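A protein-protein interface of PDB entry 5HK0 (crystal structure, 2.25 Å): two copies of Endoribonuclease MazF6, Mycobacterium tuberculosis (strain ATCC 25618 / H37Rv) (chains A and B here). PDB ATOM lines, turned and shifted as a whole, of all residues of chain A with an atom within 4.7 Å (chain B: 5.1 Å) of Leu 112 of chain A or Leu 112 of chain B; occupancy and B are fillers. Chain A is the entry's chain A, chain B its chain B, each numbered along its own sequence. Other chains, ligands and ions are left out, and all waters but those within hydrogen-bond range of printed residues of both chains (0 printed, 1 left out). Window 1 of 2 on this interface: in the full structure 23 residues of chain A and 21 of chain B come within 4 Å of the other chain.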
ATOM      1  N   ARG A   5      14.567   1.242 -27.874  1.00  0.00           N
ATOM      2  CA  ARG A   5      15.240   0.270 -27.023  1.00  0.00           C
ATOM      3  C   ARG A   5      15.690  -0.930 -27.854  1.00  0.00           C
ATOM      4  O   ARG A   5      15.202  -1.134 -28.967  1.00  0.00           O
ATOM      5  CB  ARG A   5      14.316  -0.175 -25.884  1.00  0.00           C
ATOM      6  CG  ARG A   5      15.035  -0.750 -24.671  1.00  0.00           C
ATOM      7  CD  ARG A   5      14.060  -1.062 -23.546  1.00  0.00           C
ATOM      8  NE  ARG A   5      14.745  -1.487 -22.328  1.00  0.00           N
ATOM      9  CZ  ARG A   5      14.981  -2.754 -22.004  1.00  0.00           C
ATOM     10  NH1 ARG A   5      14.584  -3.732 -22.808  1.00  0.00           N
ATOM     11  NH2 ARG A   5      15.612  -3.045 -20.875  1.00  0.00           N
ATOM     12  N   ILE A  30      19.206   0.942 -23.711  1.00  0.00           N
ATOM     13  CA  ILE A  30      18.421   0.228 -22.711  1.00  0.00           C
ATOM     14  C   ILE A  30      17.388   1.132 -22.042  1.00  0.00           C
ATOM     15  O   ILE A  30      16.641   0.688 -21.169  1.00  0.00           O
ATOM     16  CB  ILE A  30      19.323  -0.392 -21.628  1.00  0.00           C
ATOM     17  CG1 ILE A  30      20.111   0.696 -20.897  1.00  0.00           C
ATOM     18  CG2 ILE A  30      20.266  -1.415 -22.245  1.00  0.00           C
ATOM     19  CD1 ILE A  30      20.997   0.166 -19.791  1.00  0.00           C
ATOM     20  N   GLN A  31      17.349   2.397 -22.450  1.00  0.00           N
ATOM     21  CA  GLN A  31      16.333   3.319 -21.954  1.00  0.00           C
ATOM     22  C   GLN A  31      14.991   3.000 -22.603  1.00  0.00           C
ATOM     23  O   GLN A  31      14.924   2.732 -23.802  1.00  0.00           O
ATOM     24  CB  GLN A  31      16.731   4.771 -22.229  1.00  0.00           C
ATOM     25  CG  GLN A  31      15.754   5.796 -21.671  1.00  0.00           C
ATOM     26  CD  GLN A  31      16.236   7.223 -21.850  1.00  0.00           C
ATOM     27  OE1 GLN A  31      16.667   7.868 -20.895  1.00  0.00           O
ATOM     28  NE2 GLN A  31      16.159   7.726 -23.076  1.00  0.00           N
ATOM     29  N   SER A  32      13.925   3.028 -21.808  1.00  0.00           N
ATOM     30  CA  SER A  32      12.603   2.654 -22.299  1.00  0.00           C
ATOM     31  C   SER A  32      12.096   3.635 -23.350  1.00  0.00           C
ATOM     32  O   SER A  32      12.420   4.821 -23.317  1.00  0.00           O
ATOM     33  CB  SER A  32      11.602   2.567 -21.145  1.00  0.00           C
ATOM     34  OG  SER A  32      11.074   3.841 -20.832  1.00  0.00           O
ATOM     35  N   ILE A  44      20.083   6.354 -22.109  1.00  0.00           N
ATOM     36  CA  ILE A  44      20.938   5.442 -21.358  1.00  0.00           C
ATOM     37  C   ILE A  44      21.207   4.172 -22.161  1.00  0.00           C
ATOM     38  O   ILE A  44      20.290   3.589 -22.739  1.00  0.00           O
ATOM     39  CB  ILE A  44      20.300   5.078 -20.005  1.00  0.00           C
ATOM     40  CG1 ILE A  44      19.971   6.348 -19.219  1.00  0.00           C
ATOM     41  CG2 ILE A  44      21.218   4.175 -19.205  1.00  0.00           C
ATOM     42  CD1 ILE A  44      19.195   6.095 -17.951  1.00  0.00           C
ATOM     43  N   ILE A  81      27.564   1.109 -18.204  1.00  0.00           N
ATOM     44  CA  ILE A  81      26.363   1.863 -18.535  1.00  0.00           C
ATOM     45  C   ILE A  81      26.686   3.340 -18.737  1.00  0.00           C
ATOM     46  O   ILE A  81      27.319   3.968 -17.889  1.00  0.00           O
ATOM     47  CB  ILE A  81      25.291   1.713 -17.441  1.00  0.00           C
ATOM     48  CG1 ILE A  81      24.969   0.234 -17.215  1.00  0.00           C
ATOM     49  CG2 ILE A  81      24.038   2.479 -17.817  1.00  0.00           C
ATOM     50  CD1 ILE A  81      23.817  -0.004 -16.264  1.00  0.00           C
ATOM     51  N   LEU A 108      20.876  -6.856 -16.325  1.00  0.00           N
ATOM     52  CA  LEU A 108      20.709  -5.505 -15.801  1.00  0.00           C
ATOM     53  C   LEU A 108      20.076  -5.530 -14.413  1.00  0.00           C
ATOM     54  O   LEU A 108      20.434  -4.733 -13.549  1.00  0.00           O
ATOM     55  CB  LEU A 108      19.865  -4.657 -16.755  1.00  0.00           C
ATOM     56  CG  LEU A 108      20.567  -4.128 -18.009  1.00  0.00           C
ATOM     57  CD1 LEU A 108      19.563  -3.494 -18.958  1.00  0.00           C
ATOM     58  CD2 LEU A 108      21.650  -3.129 -17.634  1.00  0.00           C
ATOM     59  N   ARG A 109      19.134  -6.445 -14.203  1.00  0.00           N
ATOM     60  CA  ARG A 109      18.542  -6.624 -12.883  1.00  0.00           C
ATOM     61  C   ARG A 109      19.579  -7.161 -11.908  1.00  0.00           C
ATOM     62  O   ARG A 109      19.547  -6.853 -10.720  1.00  0.00           O
ATOM     63  CB  ARG A 109      17.351  -7.579 -12.935  1.00  0.00           C
ATOM     64  CG  ARG A 109      16.170  -7.090 -13.744  1.00  0.00           C
ATOM     65  CD  ARG A 109      14.998  -8.041 -13.591  1.00  0.00           C
ATOM     66  NE  ARG A 109      14.000  -7.852 -14.637  1.00  0.00           N
ATOM     67  CZ  ARG A 109      13.913  -8.605 -15.729  1.00  0.00           C
ATOM     68  NH1 ARG A 109      14.763  -9.606 -15.913  1.00  0.00           N
ATOM     69  NH2 ARG A 109      12.973  -8.361 -16.632  1.00  0.00           N
ATOM     70  N   ARG A 110      20.493  -7.974 -12.423  1.00  0.00           N
ATOM     71  CA  ARG A 110      21.514  -8.605 -11.600  1.00  0.00           C
ATOM     72  C   ARG A 110      22.558  -7.594 -11.140  1.00  0.00           C
ATOM     73  O   ARG A 110      22.898  -7.531  -9.959  1.00  0.00           O
ATOM     74  CB  ARG A 110      22.183  -9.746 -12.370  1.00  0.00           C
ATOM     75  CG  ARG A 110      23.135 -10.595 -11.546  1.00  0.00           C
ATOM     76  CD  ARG A 110      23.520 -11.859 -12.297  1.00  0.00           C
ATOM     77  NE  ARG A 110      24.336 -12.756 -11.485  1.00  0.00           N
ATOM     78  CZ  ARG A 110      24.712 -13.973 -11.866  1.00  0.00           C
ATOM     79  NH1 ARG A 110      24.345 -14.441 -13.051  1.00  0.00           N
ATOM     80  NH2 ARG A 110      25.456 -14.720 -11.063  1.00  0.00           N
ATOM     81  N   VAL A 111      23.061  -6.802 -12.082  1.00  0.00           N
ATOM     82  CA  VAL A 111      24.094  -5.817 -11.788  1.00  0.00           C
ATOM     83  C   VAL A 111      23.535  -4.650 -10.976  1.00  0.00           C
ATOM     84  O   VAL A 111      24.196  -4.141 -10.072  1.00  0.00           O
ATOM     85  CB  VAL A 111      24.742  -5.288 -13.086  1.00  0.00           C
ATOM     86  CG1 VAL A 111      25.731  -4.174 -12.785  1.00  0.00           C
ATOM     87  CG2 VAL A 111      25.431  -6.422 -13.826  1.00  0.00           C
ATOM     88  N   LEU A 112      22.310  -4.240 -11.288  1.00  0.00           N
ATOM     89  CA  LEU A 112      21.701  -3.095 -10.621  1.00  0.00           C
ATOM     90  C   LEU A 112      20.833  -3.497  -9.429  1.00  0.00           C
ATOM     91  O   LEU A 112      20.223  -2.640  -8.786  1.00  0.00           O
ATOM     92  CB  LEU A 112      20.867  -2.283 -11.613  1.00  0.00           C
ATOM     93  CG  LEU A 112      21.630  -1.713 -12.810  1.00  0.00           C
ATOM     94  CD1 LEU A 112      20.690  -0.948 -13.727  1.00  0.00           C
ATOM     95  CD2 LEU A 112      22.772  -0.825 -12.344  1.00  0.00           C
ATOM     96  N   ASP A 113      20.786  -4.796  -9.143  1.00  0.00           N
ATOM     97  CA  ASP A 113      20.007  -5.334  -8.026  1.00  0.00           C
ATOM     98  C   ASP A 113      18.541  -4.907  -8.107  1.00  0.00           C
ATOM     99  O   ASP A 113      18.006  -4.303  -7.178  1.00  0.00           O
ATOM    100  CB  ASP A 113      20.617  -4.899  -6.689  1.00  0.00           C
ATOM    101  CG  ASP A 113      20.052  -5.670  -5.511  1.00  0.00           C
ATOM    102  OD1 ASP A 113      19.475  -6.756  -5.731  1.00  0.00           O
ATOM    103  OD2 ASP A 113      20.188  -5.191  -4.365  1.00  0.00           O
ATOM    104  N   LEU A 114      17.900  -5.218  -9.229  1.00  0.00           N
ATOM    105  CA  LEU A 114      16.501  -4.859  -9.436  1.00  0.00           C
ATOM    106  C   LEU A 114      15.611  -6.096  -9.486  1.00  0.00           C
ATOM    107  O   LEU A 114      16.004  -7.132 -10.020  1.00  0.00           O
ATOM    108  CB  LEU A 114      16.341  -4.044 -10.721  1.00  0.00           C
ATOM    109  CG  LEU A 114      17.085  -2.708 -10.774  1.00  0.00           C
ATOM    110  CD1 LEU A 114      16.799  -1.982 -12.080  1.00  0.00           C
ATOM    111  CD2 LEU A 114      16.716  -1.838  -9.582  1.00  0.00           C
ATOM    112  N   ARG B   5      25.909  -0.633  -2.227  1.00  0.00           N
ATOM    113  CA  ARG B   5      24.715  -0.076  -2.849  1.00  0.00           C
ATOM    114  C   ARG B   5      23.950   0.812  -1.870  1.00  0.00           C
ATOM    115  O   ARG B   5      24.141   0.711  -0.656  1.00  0.00           O
ATOM    116  CB  ARG B   5      23.814  -1.203  -3.366  1.00  0.00           C
ATOM    117  CG  ARG B   5      22.769  -0.764  -4.380  1.00  0.00           C
ATOM    118  CD  ARG B   5      22.015  -1.952  -4.949  1.00  0.00           C
ATOM    119  NE  ARG B   5      21.112  -1.555  -6.026  1.00  0.00           N
ATOM    120  CZ  ARG B   5      19.833  -1.240  -5.852  1.00  0.00           C
ATOM    121  NH1 ARG B   5      19.299  -1.277  -4.639  1.00  0.00           N
ATOM    122  NH2 ARG B   5      19.088  -0.889  -6.891  1.00  0.00           N
ATOM    123  N   ILE B  30      23.956   2.338  -7.466  1.00  0.00           N
ATOM    124  CA  ILE B  30      22.812   1.485  -7.765  1.00  0.00           C
ATOM    125  C   ILE B  30      23.257   0.105  -8.234  1.00  0.00           C
ATOM    126  O   ILE B  30      22.431  -0.779  -8.457  1.00  0.00           O
ATOM    127  CB  ILE B  30      21.903   2.118  -8.835  1.00  0.00           C
ATOM    128  CG1 ILE B  30      22.696   2.398 -10.113  1.00  0.00           C
ATOM    129  CG2 ILE B  30      21.276   3.398  -8.307  1.00  0.00           C
ATOM    130  CD1 ILE B  30      21.883   3.062 -11.202  1.00  0.00           C
ATOM    131  N   GLN B  31      24.565  -0.076  -8.384  1.00  0.00           N
ATOM    132  CA  GLN B  31      25.116  -1.376  -8.742  1.00  0.00           C
ATOM    133  C   GLN B  31      25.002  -2.327  -7.555  1.00  0.00           C
ATOM    134  O   GLN B  31      25.143  -1.909  -6.406  1.00  0.00           O
ATOM    135  CB  GLN B  31      26.575  -1.242  -9.187  1.00  0.00           C
ATOM    136  CG  GLN B  31      27.178  -2.520  -9.749  1.00  0.00           C
ATOM    137  CD  GLN B  31      28.570  -2.308 -10.316  1.00  0.00           C
ATOM    138  OE1 GLN B  31      28.814  -2.549 -11.498  1.00  0.00           O
ATOM    139  NE2 GLN B  31      29.492  -1.859  -9.471  1.00  0.00           N
ATOM    140  N   SER B  32      24.740  -3.600  -7.831  1.00  0.00           N
ATOM    141  CA  SER B  32      24.566  -4.583  -6.766  1.00  0.00           C
ATOM    142  C   SER B  32      25.874  -4.826  -6.018  1.00  0.00           C
ATOM    143  O   SER B  32      26.959  -4.734  -6.591  1.00  0.00           O
ATOM    144  CB  SER B  32      24.025  -5.899  -7.326  1.00  0.00           C
ATOM    145  OG  SER B  32      24.923  -6.468  -8.258  1.00  0.00           O
ATOM    146  N   ILE B  44      28.586   1.689 -10.952  1.00  0.00           N
ATOM    147  CA  ILE B  44      27.455   2.360 -11.581  1.00  0.00           C
ATOM    148  C   ILE B  44      26.686   3.174 -10.546  1.00  0.00           C
ATOM    149  O   ILE B  44      26.362   2.672  -9.471  1.00  0.00           O
ATOM    150  CB  ILE B  44      26.507   1.354 -12.257  1.00  0.00           C
ATOM    151  CG1 ILE B  44      27.288   0.444 -13.205  1.00  0.00           C
ATOM    152  CG2 ILE B  44      25.400   2.080 -13.001  1.00  0.00           C
ATOM    153  CD1 ILE B  44      26.456  -0.655 -13.821  1.00  0.00           C
ATOM    154  N   ILE B  81      22.584   8.168 -15.639  1.00  0.00           N
ATOM    155  CA  ILE B  81      23.331   7.056 -15.066  1.00  0.00           C
ATOM    156  C   ILE B  81      24.773   7.040 -15.564  1.00  0.00           C
ATOM    157  O   ILE B  81      25.022   7.022 -16.769  1.00  0.00           O
ATOM    158  CB  ILE B  81      22.671   5.706 -15.396  1.00  0.00           C
ATOM    159  CG1 ILE B  81      21.240   5.667 -14.858  1.00  0.00           C
ATOM    160  CG2 ILE B  81      23.485   4.561 -14.822  1.00  0.00           C
ATOM    161  CD1 ILE B  81      20.555   4.334 -15.050  1.00  0.00           C
ATOM    162  N   LEU B 108      13.790   3.324 -11.451  1.00  0.00           N
ATOM    163  CA  LEU B 108      14.871   2.744 -12.238  1.00  0.00           C
ATOM    164  C   LEU B 108      14.323   1.751 -13.257  1.00  0.00           C
ATOM    165  O   LEU B 108      14.870   1.597 -14.348  1.00  0.00           O
ATOM    166  CB  LEU B 108      15.886   2.055 -11.325  1.00  0.00           C
ATOM    167  CG  LEU B 108      17.367   2.286 -11.618  1.00  0.00           C
ATOM    168  CD1 LEU B 108      17.683   3.772 -11.628  1.00  0.00           C
ATOM    169  CD2 LEU B 108      18.223   1.564 -10.591  1.00  0.00           C
ATOM    170  N   ARG B 109      13.235   1.079 -12.893  1.00  0.00           N
ATOM    171  CA  ARG B 109      12.621   0.086 -13.763  1.00  0.00           C
ATOM    172  C   ARG B 109      11.792   0.730 -14.869  1.00  0.00           C
ATOM    173  O   ARG B 109      11.648   0.166 -15.951  1.00  0.00           O
ATOM    174  CB  ARG B 109      11.749  -0.872 -12.951  1.00  0.00           C
ATOM    175  CG  ARG B 109      12.533  -1.759 -12.000  1.00  0.00           C
ATOM    176  CD  ARG B 109      11.651  -2.835 -11.394  1.00  0.00           C
ATOM    177  NE  ARG B 109      12.285  -3.469 -10.242  1.00  0.00           N
ATOM    178  CZ  ARG B 109      12.027  -3.146  -8.979  1.00  0.00           C
ATOM    179  NH1 ARG B 109      11.141  -2.200  -8.701  1.00  0.00           N
ATOM    180  NH2 ARG B 109      12.651  -3.773  -7.991  1.00  0.00           N
ATOM    181  N   ARG B 110      11.244   1.909 -14.594  1.00  0.00           N
ATOM    182  CA  ARG B 110      10.482   2.641 -15.601  1.00  0.00           C
ATOM    183  C   ARG B 110      11.394   3.164 -16.704  1.00  0.00           C
ATOM    184  O   ARG B 110      11.074   3.065 -17.889  1.00  0.00           O
ATOM    185  CB  ARG B 110       9.719   3.804 -14.965  1.00  0.00           C
ATOM    186  CG  ARG B 110       8.373   3.428 -14.370  1.00  0.00           C
ATOM    187  CD  ARG B 110       7.628   4.669 -13.899  1.00  0.00           C
ATOM    188  NE  ARG B 110       6.276   4.362 -13.438  1.00  0.00           N
ATOM    189  CZ  ARG B 110       5.424   5.269 -12.970  1.00  0.00           C
ATOM    190  NH1 ARG B 110       5.785   6.544 -12.898  1.00  0.00           N
ATOM    191  NH2 ARG B 110       4.213   4.903 -12.573  1.00  0.00           N
ATOM    192  N   VAL B 111      12.532   3.720 -16.303  1.00  0.00           N
ATOM    193  CA  VAL B 111      13.474   4.324 -17.237  1.00  0.00           C
ATOM    194  C   VAL B 111      14.180   3.280 -18.099  1.00  0.00           C
ATOM    195  O   VAL B 111      14.435   3.507 -19.282  1.00  0.00           O
ATOM    196  CB  VAL B 111      14.528   5.163 -16.486  1.00  0.00           C
ATOM    197  CG1 VAL B 111      15.547   5.747 -17.451  1.00  0.00           C
ATOM    198  CG2 VAL B 111      13.848   6.269 -15.702  1.00  0.00           C
ATOM    199  N   LEU B 112      14.482   2.128 -17.510  1.00  0.00           N
ATOM    200  CA  LEU B 112      15.234   1.096 -18.213  1.00  0.00           C
ATOM    201  C   LEU B 112      14.333  -0.015 -18.735  1.00  0.00           C
ATOM    202  O   LEU B 112      14.816  -1.022 -19.254  1.00  0.00           O
ATOM    203  CB  LEU B 112      16.301   0.506 -17.294  1.00  0.00           C
ATOM    204  CG  LEU B 112      17.271   1.525 -16.699  1.00  0.00           C
ATOM    205  CD1 LEU B 112      18.274   0.839 -15.792  1.00  0.00           C
ATOM    206  CD2 LEU B 112      17.977   2.299 -17.802  1.00  0.00           C
ATOM    207  N   ASP B 113      13.024   0.180 -18.594  1.00  0.00           N
ATOM    208  CA  ASP B 113      12.032  -0.829 -18.957  1.00  0.00           C
ATOM    209  C   ASP B 113      12.321  -2.183 -18.291  1.00  0.00           C
ATOM    210  O   ASP B 113      12.233  -3.231 -18.932  1.00  0.00           O
ATOM    211  CB  ASP B 113      11.956  -0.983 -20.483  1.00  0.00           C
ATOM    212  CG  ASP B 113      10.563  -0.707 -21.030  1.00  0.00           C
ATOM    213  OD1 ASP B 113       9.765  -0.055 -20.324  1.00  0.00           O
ATOM    214  OD2 ASP B 113      10.262  -1.137 -22.165  1.00  0.00           O
ATOM    215  N   LEU B 114      12.669  -2.144 -17.005  1.00  0.00           N
ATOM    216  CA  LEU B 114      12.898  -3.348 -16.206  1.00  0.00           C
ATOM    217  C   LEU B 114      11.828  -3.471 -15.134  1.00  0.00           C
ATOM    218  O   LEU B 114      11.023  -4.390 -15.139  1.00  0.00           O
ATOM    219  CB  LEU B 114      14.283  -3.317 -15.554  1.00  0.00           C
ATOM    220  CG  LEU B 114      15.474  -3.202 -16.508  1.00  0.00           C
ATOM    221  CD1 LEU B 114      16.747  -3.042 -15.707  1.00  0.00           C
ATOM    222  CD2 LEU B 114      15.538  -4.422 -17.407  1.00  0.00           C
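The backbone carbonyl oxygen of Leu 112 of chain B sits close to the backbone carbonyl oxygen of Ile 30 of chain A (3.1 Å).
N of Ser 32 of chain A lies within hydrogen-bond range of O of Val 111 of chain B (2.6 Å).
The backbone carbonyl oxygen of Arg 110 of chain A lies within hydrogen-bond range of the side-chain hydroxyl of Ser 32 of chain B (2.9 Å).
OG of Ser 32 of chain B is in hydrogen-bond range of O of Val 111 of chain A (3.0 Å).
The guanidinium group of Arg 5 of chain B sits at hydrogen-bond distance from the backbone carbonyl oxygen of Leu 112 of chain A (2.8 Å).
The backbone carbonyl oxygen (O) of Arg 110 of chain B is in hydrogen-bond range of the side-chain hydroxyl (OG) of Ser 32 of chain A, at 3.0 Å.
The guanidinium group (NH2) of Arg 5 of chain A sits at hydrogen-bond distance from the backbone carbonyl oxygen (O) of Leu 112 of chain B, 2.7 Å away.
The backbone carbonyl oxygen of Leu 112 of chain A sits close to the backbone carbonyl oxygen of Ile 30 of chain B.
Printed residues of chain B within 4 Å of Leu 108 of chain A: Leu 114.
Arg 109 of chain A touches none of the printed residues of chain B.
Of the printed residues of chain B, Val 111 of chain A touches Gln 31, Ser 32 and Ile 44.
Of chain B, only Arg 5 (2.8 Å), Ile 30 (2.9 Å), Ile 44 (3.97 Å) and Leu 112 (3.6 Å) come within 4 Å of Leu 112 of chain A.
Of the printed residues of chain A, Ser 32 of chain B touches Arg 110 (2.9 Å), Val 111 (2.4 Å) and Asp 113 (3.6 Å).
Arg 109 of chain B touches none of the printed residues of chain A.
Printed residues of chain A within 4 Å of Leu 112 of chain B: Arg 5, Ile 30, Ile 44 and Leu 112.
Of the printed residues of chain A, Leu 114 of chain B touches Arg 5 (3.7 Å), Leu 108 (3.7 Å) and Leu 114 (3.8 Å).
The nearest residue of chain B that does not touch Leu 112 of chain A is Ser 32 of chain B (4.2 Å).
Ser 32 of chain A touches Val 111 of chain B, and with the chains exchanged Val 111 of chain A touches Ser 32 of chain B.
Ile 44 of chain A touches Leu 112 of chain B, and with the chains exchanged Leu 112 of chain A touches Ile 44 of chain B.
Ile 81 of chain A touches its own counterpart, Ile 81 of chain B.
Leu 108 of chain A touches Leu 114 of chain B, and with the chains exchanged Leu 114 of chain A touches Leu 108 of chain B.
The guanidinium group (NE) of Arg 5 of chain B lies within hydrogen-bond range of the backbone carbonyl oxygen (O) of Ile 30 of chain B (2.9 Å).
The backbone NH of Gln 31 of chain B sits at hydrogen-bond distance from the backbone carbonyl oxygen of Ile 44 of chain B, at 3.5 Å.
The backbone NH (N) of Leu 114 of chain A sits at hydrogen-bond distance from the backbone carbonyl oxygen (O) of Arg 109 of chain A, at 2.8 Å.
N of Leu 114 of chain B sits at hydrogen-bond distance from O of Arg 109 of chain B, at 2.7 Å.
O of Ile 30 of chain A sits at hydrogen-bond distance from NE of Arg 5 of chain A, at 3.1 Å.
The backbone NH of Ile 30 of chain B sits at hydrogen-bond distance from the backbone carbonyl oxygen of Ile 44 of chain B (3.1 Å).
Hydrophobic or aromatic side chains of chain A that line the printed part of chain B: Ile 44, Ile 81, Leu 108, Val 111, Leu 112 and Leu 114.
Of the 13 printed residues of chain B, 12 touch a printed residue of chain A.
Hydrophobic or aromatic side chains of chain B that line the printed part of chain A: Ile 30, Ile 44, Ile 81, Leu 108, Val 111, Leu 112 and Leu 114.
Among the printed residues, 27 pairs touch across the chains.
Among the printed residues, no Asp or Glu carboxylate lies within 4 Å of a Lys or Arg side-chain nitrogen of the other chain.
Among the printed residues, pairs that only touch across the chains: Arg 5 of chain A with Asp 113 of chain B (3.4 Å), Arg 5 of chain A with Leu 114 of chain B (3.7 Å), Gln 31 of chain A with Val 111 of chain B (3.3 Å), Ser 32 of chain A with Asp 113 of chain B (3.3 Å), Ile 44 of chain A with Ile 81 of chain B (3.7 Å), Ile 44 of chain A with Val 111 of chain B (3.7 Å), Ile 44 of chain A with Leu 112 of chain B (3.99 Å), Ile 81 of chain A with Ile 44 of chain B (3.7 Å), Ile 81 of chain A with Ile 81 of chain B (3.7 Å), Leu 108 of chain A with Leu 114 of chain B (3.7 Å), Val 111 of chain A with Gln 31 of chain B (3.2 Å), Val 111 of chain A with Ile 44 of chain B (3.7 Å), Leu 112 of chain A with Ile 44 of chain B (3.97 Å), Leu 112 of chain A with Leu 112 of chain B (3.6 Å), Asp 113 of chain A with Arg 5 of chain B (3.4 Å), Asp 113 of chain A with Ser 32 of chain B (3.6 Å), Leu 114 of chain A with Arg 5 of chain B (3.7 Å), Leu 114 of chain A with Leu 108 of chain B (3.9 Å) and Leu 114 of chain A with Leu 114 of chain B (3.8 Å).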
